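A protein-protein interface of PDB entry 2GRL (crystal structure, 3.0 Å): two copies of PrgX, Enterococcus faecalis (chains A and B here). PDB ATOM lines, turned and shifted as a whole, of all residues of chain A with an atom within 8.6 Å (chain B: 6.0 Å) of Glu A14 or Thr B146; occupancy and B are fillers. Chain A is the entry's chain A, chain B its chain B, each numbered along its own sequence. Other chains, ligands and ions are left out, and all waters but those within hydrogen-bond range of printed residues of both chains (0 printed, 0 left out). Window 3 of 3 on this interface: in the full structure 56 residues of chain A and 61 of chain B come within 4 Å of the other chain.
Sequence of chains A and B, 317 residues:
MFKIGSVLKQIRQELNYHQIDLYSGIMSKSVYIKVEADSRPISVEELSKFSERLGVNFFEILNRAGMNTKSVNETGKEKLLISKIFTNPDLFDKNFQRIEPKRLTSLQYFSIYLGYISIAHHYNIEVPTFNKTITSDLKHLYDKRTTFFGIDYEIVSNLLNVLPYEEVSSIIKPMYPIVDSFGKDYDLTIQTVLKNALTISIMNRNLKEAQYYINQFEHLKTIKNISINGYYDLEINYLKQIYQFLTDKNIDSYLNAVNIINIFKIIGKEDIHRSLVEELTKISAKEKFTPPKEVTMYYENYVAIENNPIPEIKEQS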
ATOM      1  N   VAL A   7      -1.963 -29.918  -3.091  1.00  0.00           N
ATOM      2  CA  VAL A   7      -0.722 -30.243  -3.776  1.00  0.00           C
ATOM      3  C   VAL A   7      -1.156 -30.951  -5.069  1.00  0.00           C
ATOM      4  O   VAL A   7      -0.645 -30.661  -6.159  1.00  0.00           O
ATOM      5  CB  VAL A   7       0.188 -31.173  -2.930  1.00  0.00           C
ATOM      6  CG1 VAL A   7       1.367 -31.651  -3.758  1.00  0.00           C
ATOM      7  CG2 VAL A   7       0.687 -30.445  -1.705  1.00  0.00           C
ATOM      8  N   LEU A   8      -2.125 -31.856  -4.951  1.00  0.00           N
ATOM      9  CA  LEU A   8      -2.626 -32.575  -6.121  1.00  0.00           C
ATOM     10  C   LEU A   8      -3.089 -31.581  -7.183  1.00  0.00           C
ATOM     11  O   LEU A   8      -2.648 -31.634  -8.331  1.00  0.00           O
ATOM     12  CB  LEU A   8      -3.780 -33.510  -5.738  1.00  0.00           C
ATOM     13  CG  LEU A   8      -3.376 -34.753  -4.949  1.00  0.00           C
ATOM     14  CD1 LEU A   8      -4.624 -35.534  -4.579  1.00  0.00           C
ATOM     15  CD2 LEU A   8      -2.416 -35.632  -5.781  1.00  0.00           C
ATOM     16  N   LYS A   9      -3.978 -30.673  -6.794  1.00  0.00           N
ATOM     17  CA  LYS A   9      -4.488 -29.666  -7.711  1.00  0.00           C
ATOM     18  C   LYS A   9      -3.345 -28.854  -8.312  1.00  0.00           C
ATOM     19  O   LYS A   9      -3.356 -28.541  -9.505  1.00  0.00           O
ATOM     20  CB  LYS A   9      -5.447 -28.729  -6.979  1.00  0.00           C
ATOM     21  CG  LYS A   9      -5.464 -27.339  -7.568  1.00  0.00           C
ATOM     22  CD  LYS A   9      -6.359 -26.401  -6.805  1.00  0.00           C
ATOM     23  CE  LYS A   9      -7.814 -26.605  -7.176  1.00  0.00           C
ATOM     24  NZ  LYS A   9      -8.633 -25.450  -6.723  1.00  0.00           N
ATOM     25  N   GLN A  10      -2.368 -28.520  -7.474  1.00  0.00           N
ATOM     26  CA  GLN A  10      -1.217 -27.743  -7.908  1.00  0.00           C
ATOM     27  C   GLN A  10      -0.450 -28.452  -9.023  1.00  0.00           C
ATOM     28  O   GLN A  10      -0.187 -27.877 -10.084  1.00  0.00           O
ATOM     29  CB  GLN A  10      -0.298 -27.492  -6.723  1.00  0.00           C
ATOM     30  CG  GLN A  10       1.094 -27.067  -7.110  1.00  0.00           C
ATOM     31  CD  GLN A  10       1.949 -26.779  -5.906  1.00  0.00           C
ATOM     32  OE1 GLN A  10       3.164 -26.610  -6.020  1.00  0.00           O
ATOM     33  NE2 GLN A  10       1.319 -26.710  -4.734  1.00  0.00           N
ATOM     34  N   ILE A  11      -0.098 -29.705  -8.766  1.00  0.00           N
ATOM     35  CA  ILE A  11       0.632 -30.506  -9.727  1.00  0.00           C
ATOM     36  C   ILE A  11      -0.254 -30.766 -10.953  1.00  0.00           C
ATOM     37  O   ILE A  11       0.192 -30.671 -12.105  1.00  0.00           O
ATOM     38  CB  ILE A  11       1.044 -31.842  -9.082  1.00  0.00           C
ATOM     39  CG1 ILE A  11       1.874 -31.560  -7.829  1.00  0.00           C
ATOM     40  CG2 ILE A  11       1.852 -32.675 -10.063  1.00  0.00           C
ATOM     41  CD1 ILE A  11       2.269 -32.810  -7.078  1.00  0.00           C
ATOM     42  N   ARG A  12      -1.514 -31.090 -10.689  1.00  0.00           N
ATOM     43  CA  ARG A  12      -2.478 -31.374 -11.738  1.00  0.00           C
ATOM     44  C   ARG A  12      -2.522 -30.233 -12.736  1.00  0.00           C
ATOM     45  O   ARG A  12      -2.574 -30.452 -13.957  1.00  0.00           O
ATOM     46  CB  ARG A  12      -3.871 -31.553 -11.143  1.00  0.00           C
ATOM     47  CG  ARG A  12      -4.856 -32.255 -12.063  1.00  0.00           C
ATOM     48  CD  ARG A  12      -6.258 -31.981 -11.612  1.00  0.00           C
ATOM     49  NE  ARG A  12      -6.750 -30.753 -12.227  1.00  0.00           N
ATOM     50  CZ  ARG A  12      -7.497 -29.844 -11.607  1.00  0.00           C
ATOM     51  NH1 ARG A  12      -7.834 -30.016 -10.342  1.00  0.00           N
ATOM     52  NH2 ARG A  12      -7.932 -28.776 -12.269  1.00  0.00           N
ATOM     53  N   GLN A  13      -2.505 -29.011 -12.210  1.00  0.00           N
ATOM     54  CA  GLN A  13      -2.556 -27.816 -13.048  1.00  0.00           C
ATOM     55  C   GLN A  13      -1.238 -27.456 -13.733  1.00  0.00           C
ATOM     56  O   GLN A  13      -1.219 -27.017 -14.883  1.00  0.00           O
ATOM     57  CB  GLN A  13      -3.070 -26.650 -12.223  1.00  0.00           C
ATOM     58  CG  GLN A  13      -4.543 -26.821 -11.857  1.00  0.00           C
ATOM     59  CD  GLN A  13      -5.081 -25.750 -10.908  1.00  0.00           C
ATOM     60  OE1 GLN A  13      -6.287 -25.673 -10.682  1.00  0.00           O
ATOM     61  NE2 GLN A  13      -4.189 -24.933 -10.341  1.00  0.00           N
ATOM     62  N   GLU A  14      -0.129 -27.643 -13.035  1.00  0.00           N
ATOM     63  CA  GLU A  14       1.153 -27.345 -13.639  1.00  0.00           C
ATOM     64  C   GLU A  14       1.314 -28.227 -14.874  1.00  0.00           C
ATOM     65  O   GLU A  14       1.832 -27.790 -15.898  1.00  0.00           O
ATOM     66  CB  GLU A  14       2.284 -27.622 -12.647  1.00  0.00           C
ATOM     67  CG  GLU A  14       3.673 -27.543 -13.264  1.00  0.00           C
ATOM     68  CD  GLU A  14       4.004 -26.159 -13.782  1.00  0.00           C
ATOM     69  OE1 GLU A  14       4.952 -26.014 -14.578  1.00  0.00           O
ATOM     70  OE2 GLU A  14       3.315 -25.206 -13.383  1.00  0.00           O
ATOM     71  N   LEU A  15       0.860 -29.472 -14.777  1.00  0.00           N
ATOM     72  CA  LEU A  15       0.980 -30.408 -15.882  1.00  0.00           C
ATOM     73  C   LEU A  15      -0.173 -30.338 -16.874  1.00  0.00           C
ATOM     74  O   LEU A  15      -0.222 -31.110 -17.832  1.00  0.00           O
ATOM     75  CB  LEU A  15       1.125 -31.821 -15.319  1.00  0.00           C
ATOM     76  CG  LEU A  15       2.550 -32.310 -15.015  1.00  0.00           C
ATOM     77  CD1 LEU A  15       3.475 -31.182 -14.580  1.00  0.00           C
ATOM     78  CD2 LEU A  15       2.458 -33.386 -13.939  1.00  0.00           C
ATOM     79  N   ASN A  16      -1.096 -29.405 -16.638  1.00  0.00           N
ATOM     80  CA  ASN A  16      -2.267 -29.199 -17.493  1.00  0.00           C
ATOM     81  C   ASN A  16      -3.183 -30.400 -17.623  1.00  0.00           C
ATOM     82  O   ASN A  16      -3.602 -30.736 -18.726  1.00  0.00           O
ATOM     83  CB  ASN A  16      -1.852 -28.763 -18.900  1.00  0.00           C
ATOM     84  CG  ASN A  16      -1.069 -27.479 -18.898  1.00  0.00           C
ATOM     85  OD1 ASN A  16      -1.415 -26.531 -18.191  1.00  0.00           O
ATOM     86  ND2 ASN A  16      -0.005 -27.429 -19.699  1.00  0.00           N
ATOM     87  N   TYR A  17      -3.489 -31.057 -16.509  1.00  0.00           N
ATOM     88  CA  TYR A  17      -4.394 -32.206 -16.537  1.00  0.00           C
ATOM     89  C   TYR A  17      -5.743 -31.711 -16.030  1.00  0.00           C
ATOM     90  O   TYR A  17      -5.806 -30.750 -15.266  1.00  0.00           O
ATOM     91  CB  TYR A  17      -3.897 -33.326 -15.612  1.00  0.00           C
ATOM     92  CG  TYR A  17      -2.705 -34.117 -16.111  1.00  0.00           C
ATOM     93  CD1 TYR A  17      -2.777 -34.865 -17.286  1.00  0.00           C
ATOM     94  CD2 TYR A  17      -1.521 -34.163 -15.373  1.00  0.00           C
ATOM     95  CE1 TYR A  17      -1.693 -35.647 -17.714  1.00  0.00           C
ATOM     96  CE2 TYR A  17      -0.440 -34.941 -15.785  1.00  0.00           C
ATOM     97  CZ  TYR A  17      -0.528 -35.682 -16.956  1.00  0.00           C
ATOM     98  OH  TYR A  17       0.538 -36.461 -17.356  1.00  0.00           O
ATOM     99  N   LEU A  54      -0.540 -38.456 -12.323  1.00  0.00           N
ATOM    100  CA  LEU A  54       0.249 -37.244 -12.476  1.00  0.00           C
ATOM    101  C   LEU A  54       1.672 -37.467 -12.984  1.00  0.00           C
ATOM    102  O   LEU A  54       2.296 -36.539 -13.505  1.00  0.00           O
ATOM    103  CB  LEU A  54       0.293 -36.505 -11.144  1.00  0.00           C
ATOM    104  CG  LEU A  54      -1.043 -35.926 -10.686  1.00  0.00           C
ATOM    105  CD1 LEU A  54      -0.969 -35.617  -9.205  1.00  0.00           C
ATOM    106  CD2 LEU A  54      -1.367 -34.682 -11.499  1.00  0.00           C
ATOM    107  N   VAL A  56       4.148 -37.954 -11.171  1.00  0.00           N
ATOM    108  CA  VAL A  56       5.029 -37.398 -10.164  1.00  0.00           C
ATOM    109  C   VAL A  56       5.164 -38.353  -8.984  1.00  0.00           C
ATOM    110  O   VAL A  56       4.192 -38.971  -8.578  1.00  0.00           O
ATOM    111  CB  VAL A  56       4.487 -36.053  -9.655  1.00  0.00           C
ATOM    112  CG1 VAL A  56       5.332 -35.571  -8.463  1.00  0.00           C
ATOM    113  CG2 VAL A  56       4.507 -35.033 -10.784  1.00  0.00           C
ATOM    114  N   LYS B 144       5.459 -23.660 -21.071  1.00  0.00           N
ATOM    115  CA  LYS B 144       4.748 -22.873 -20.083  1.00  0.00           C
ATOM    116  C   LYS B 144       4.809 -23.464 -18.672  1.00  0.00           C
ATOM    117  O   LYS B 144       3.822 -23.474 -17.946  1.00  0.00           O
ATOM    118  CB  LYS B 144       3.308 -22.683 -20.545  1.00  0.00           C
ATOM    119  CG  LYS B 144       3.223 -22.194 -21.991  1.00  0.00           C
ATOM    120  CD  LYS B 144       1.851 -21.635 -22.335  1.00  0.00           C
ATOM    121  CE  LYS B 144       1.580 -20.346 -21.571  1.00  0.00           C
ATOM    122  NZ  LYS B 144       0.227 -19.798 -21.857  1.00  0.00           N
ATOM    123  N   ARG B 145       5.981 -23.958 -18.292  1.00  0.00           N
ATOM    124  CA  ARG B 145       6.188 -24.526 -16.965  1.00  0.00           C
ATOM    125  C   ARG B 145       6.675 -23.407 -16.055  1.00  0.00           C
ATOM    126  O   ARG B 145       7.243 -22.421 -16.531  1.00  0.00           O
ATOM    127  CB  ARG B 145       7.233 -25.653 -17.012  1.00  0.00           C
ATOM    128  CG  ARG B 145       6.760 -26.923 -17.697  1.00  0.00           C
ATOM    129  CD  ARG B 145       5.541 -27.492 -16.996  1.00  0.00           C
ATOM    130  NE  ARG B 145       5.827 -27.896 -15.623  1.00  0.00           N
ATOM    131  CZ  ARG B 145       6.505 -28.987 -15.270  1.00  0.00           C
ATOM    132  NH1 ARG B 145       6.970 -29.810 -16.201  1.00  0.00           N
ATOM    133  NH2 ARG B 145       6.739 -29.241 -13.984  1.00  0.00           N
ATOM    134  N   THR B 146       6.448 -23.558 -14.751  1.00  0.00           N
ATOM    135  CA  THR B 146       6.863 -22.543 -13.791  1.00  0.00           C
ATOM    136  C   THR B 146       7.420 -23.148 -12.513  1.00  0.00           C
ATOM    137  O   THR B 146       8.167 -22.497 -11.795  1.00  0.00           O
ATOM    138  CB  THR B 146       5.689 -21.648 -13.409  1.00  0.00           C
ATOM    139  OG1 THR B 146       4.757 -22.403 -12.632  1.00  0.00           O
ATOM    140  CG2 THR B 146       4.983 -21.147 -14.641  1.00  0.00           C
ATOM    141  N   THR B 147       7.040 -24.387 -12.228  1.00  0.00           N
ATOM    142  CA  THR B 147       7.498 -25.084 -11.030  1.00  0.00           C
ATOM    143  C   THR B 147       7.944 -26.464 -11.465  1.00  0.00           C
ATOM    144  O   THR B 147       7.301 -27.074 -12.319  1.00  0.00           O
ATOM    145  CB  THR B 147       6.374 -25.249 -10.015  1.00  0.00           C
ATOM    146  OG1 THR B 147       5.789 -23.973  -9.754  1.00  0.00           O
ATOM    147  CG2 THR B 147       6.913 -25.822  -8.718  1.00  0.00           C
ATOM    148  N   PHE B 148       9.027 -26.971 -10.883  1.00  0.00           N
ATOM    149  CA  PHE B 148       9.518 -28.273 -11.296  1.00  0.00           C
ATOM    150  C   PHE B 148       9.584 -29.314 -10.208  1.00  0.00           C
ATOM    151  O   PHE B 148       9.867 -29.026  -9.038  1.00  0.00           O
ATOM    152  CB  PHE B 148      10.875 -28.107 -11.966  1.00  0.00           C
ATOM    153  CG  PHE B 148      10.872 -27.050 -13.028  1.00  0.00           C
ATOM    154  CD1 PHE B 148      11.116 -25.717 -12.707  1.00  0.00           C
ATOM    155  CD2 PHE B 148      10.528 -27.369 -14.335  1.00  0.00           C
ATOM    156  CE1 PHE B 148      11.010 -24.719 -13.668  1.00  0.00           C
ATOM    157  CE2 PHE B 148      10.418 -26.381 -15.297  1.00  0.00           C
ATOM    158  CZ  PHE B 148      10.659 -25.050 -14.964  1.00  0.00           C
ATOM    159  N   PHE B 149       9.310 -30.544 -10.614  1.00  0.00           N
ATOM    160  CA  PHE B 149       9.320 -31.673  -9.702  1.00  0.00           C
ATOM    161  C   PHE B 149      10.506 -32.578  -9.996  1.00  0.00           C
ATOM    162  O   PHE B 149      11.198 -32.418 -11.008  1.00  0.00           O
ATOM    163  CB  PHE B 149       8.011 -32.443  -9.824  1.00  0.00           C
ATOM    164  CG  PHE B 149       6.805 -31.559  -9.856  1.00  0.00           C
ATOM    165  CD1 PHE B 149       6.289 -31.107 -11.072  1.00  0.00           C
ATOM    166  CD2 PHE B 149       6.214 -31.121  -8.673  1.00  0.00           C
ATOM    167  CE1 PHE B 149       5.196 -30.227 -11.110  1.00  0.00           C
ATOM    168  CE2 PHE B 149       5.128 -30.245  -8.698  1.00  0.00           C
ATOM    169  CZ  PHE B 149       4.615 -29.798  -9.919  1.00  0.00           C
ATOM    170  N   PRO B 174      16.088 -22.115 -15.939  1.00  0.00           N
ATOM    171  CA  PRO B 174      14.951 -21.724 -15.098  1.00  0.00           C
ATOM    172  C   PRO B 174      14.598 -22.705 -13.963  1.00  0.00           C
ATOM    173  O   PRO B 174      13.731 -22.415 -13.132  1.00  0.00           O
ATOM    174  CB  PRO B 174      13.820 -21.563 -16.109  1.00  0.00           C
ATOM    175  CG  PRO B 174      14.144 -22.581 -17.130  1.00  0.00           C
ATOM    176  CD  PRO B 174      15.643 -22.435 -17.307  1.00  0.00           C
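Phe B149 touches Ile A11. Glu A14 touches Phe B149. CD1 of Leu A15 touches CZ of Arg B145 (3.8 Å). CD1 of Leu A15 touches CE1 of Phe B149 (3.99 Å).
The guanidinium group (NH2) of Arg B145 is in salt-bridge range of the side-chain carboxylate (OE1) of Glu A14, at 3.7 Å. OE1 of Glu A14 is in hydrogen-bond range of N of Thr B146, 2.9 Å away. The side-chain carboxylate (OE1) of Glu A14 sits close to the backbone carbonyl oxygen (O) of Thr B147 (3.4 Å).
Printed residues of chain B within 4 Å of Ile A11: Phe B149. Glu A14 touches four residues of chain B. Of the printed residues of chain B, Leu A15 touches Arg B145 (3.8 Å) and Phe B149 (3.99 Å). Lys B144 touches none of the printed residues of chain A. Of the printed residues of chain A, Arg B145 touches Glu A14 and Leu A15. Thr B146 touches just one residue of chain A: Glu A14 (2.9 Å). Of the printed residues of chain A, Phe B149 touches Ile A11, Glu A14 and Leu A15. The nearest residue of chain B that does not touch Glu A14 is Lys B144 (4.4 Å). The nearest printed residue of chain A that does not touch Arg B145 is Asn A16 (6.2 Å).
Of the 7 printed residues of chain B, 4 touch a printed residue of chain A. Printed residues of chain B that touch a printed residue of chain A: Arg B145, Thr B146, Thr B147 and Phe B149. Hydrophobic or aromatic side chains of chain B within 4 Å of the printed part of chain A: Phe B149. Along chain B the printed residues that touch a printed residue of chain A span positions 145 to 149.
The guanidinium group of Arg B145 lies within hydrogen-bond range of the backbone carbonyl oxygen of Thr B147 (2.8 Å). The side-chain hydroxyl (OG1) of Thr B146 sits close to the side-chain hydroxyl (OG1) of Thr B147.
No position is printed for both chains. Of the 7 pairs that touch across the chains among the printed residues, none has its exchanged pair printed and touching as well.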
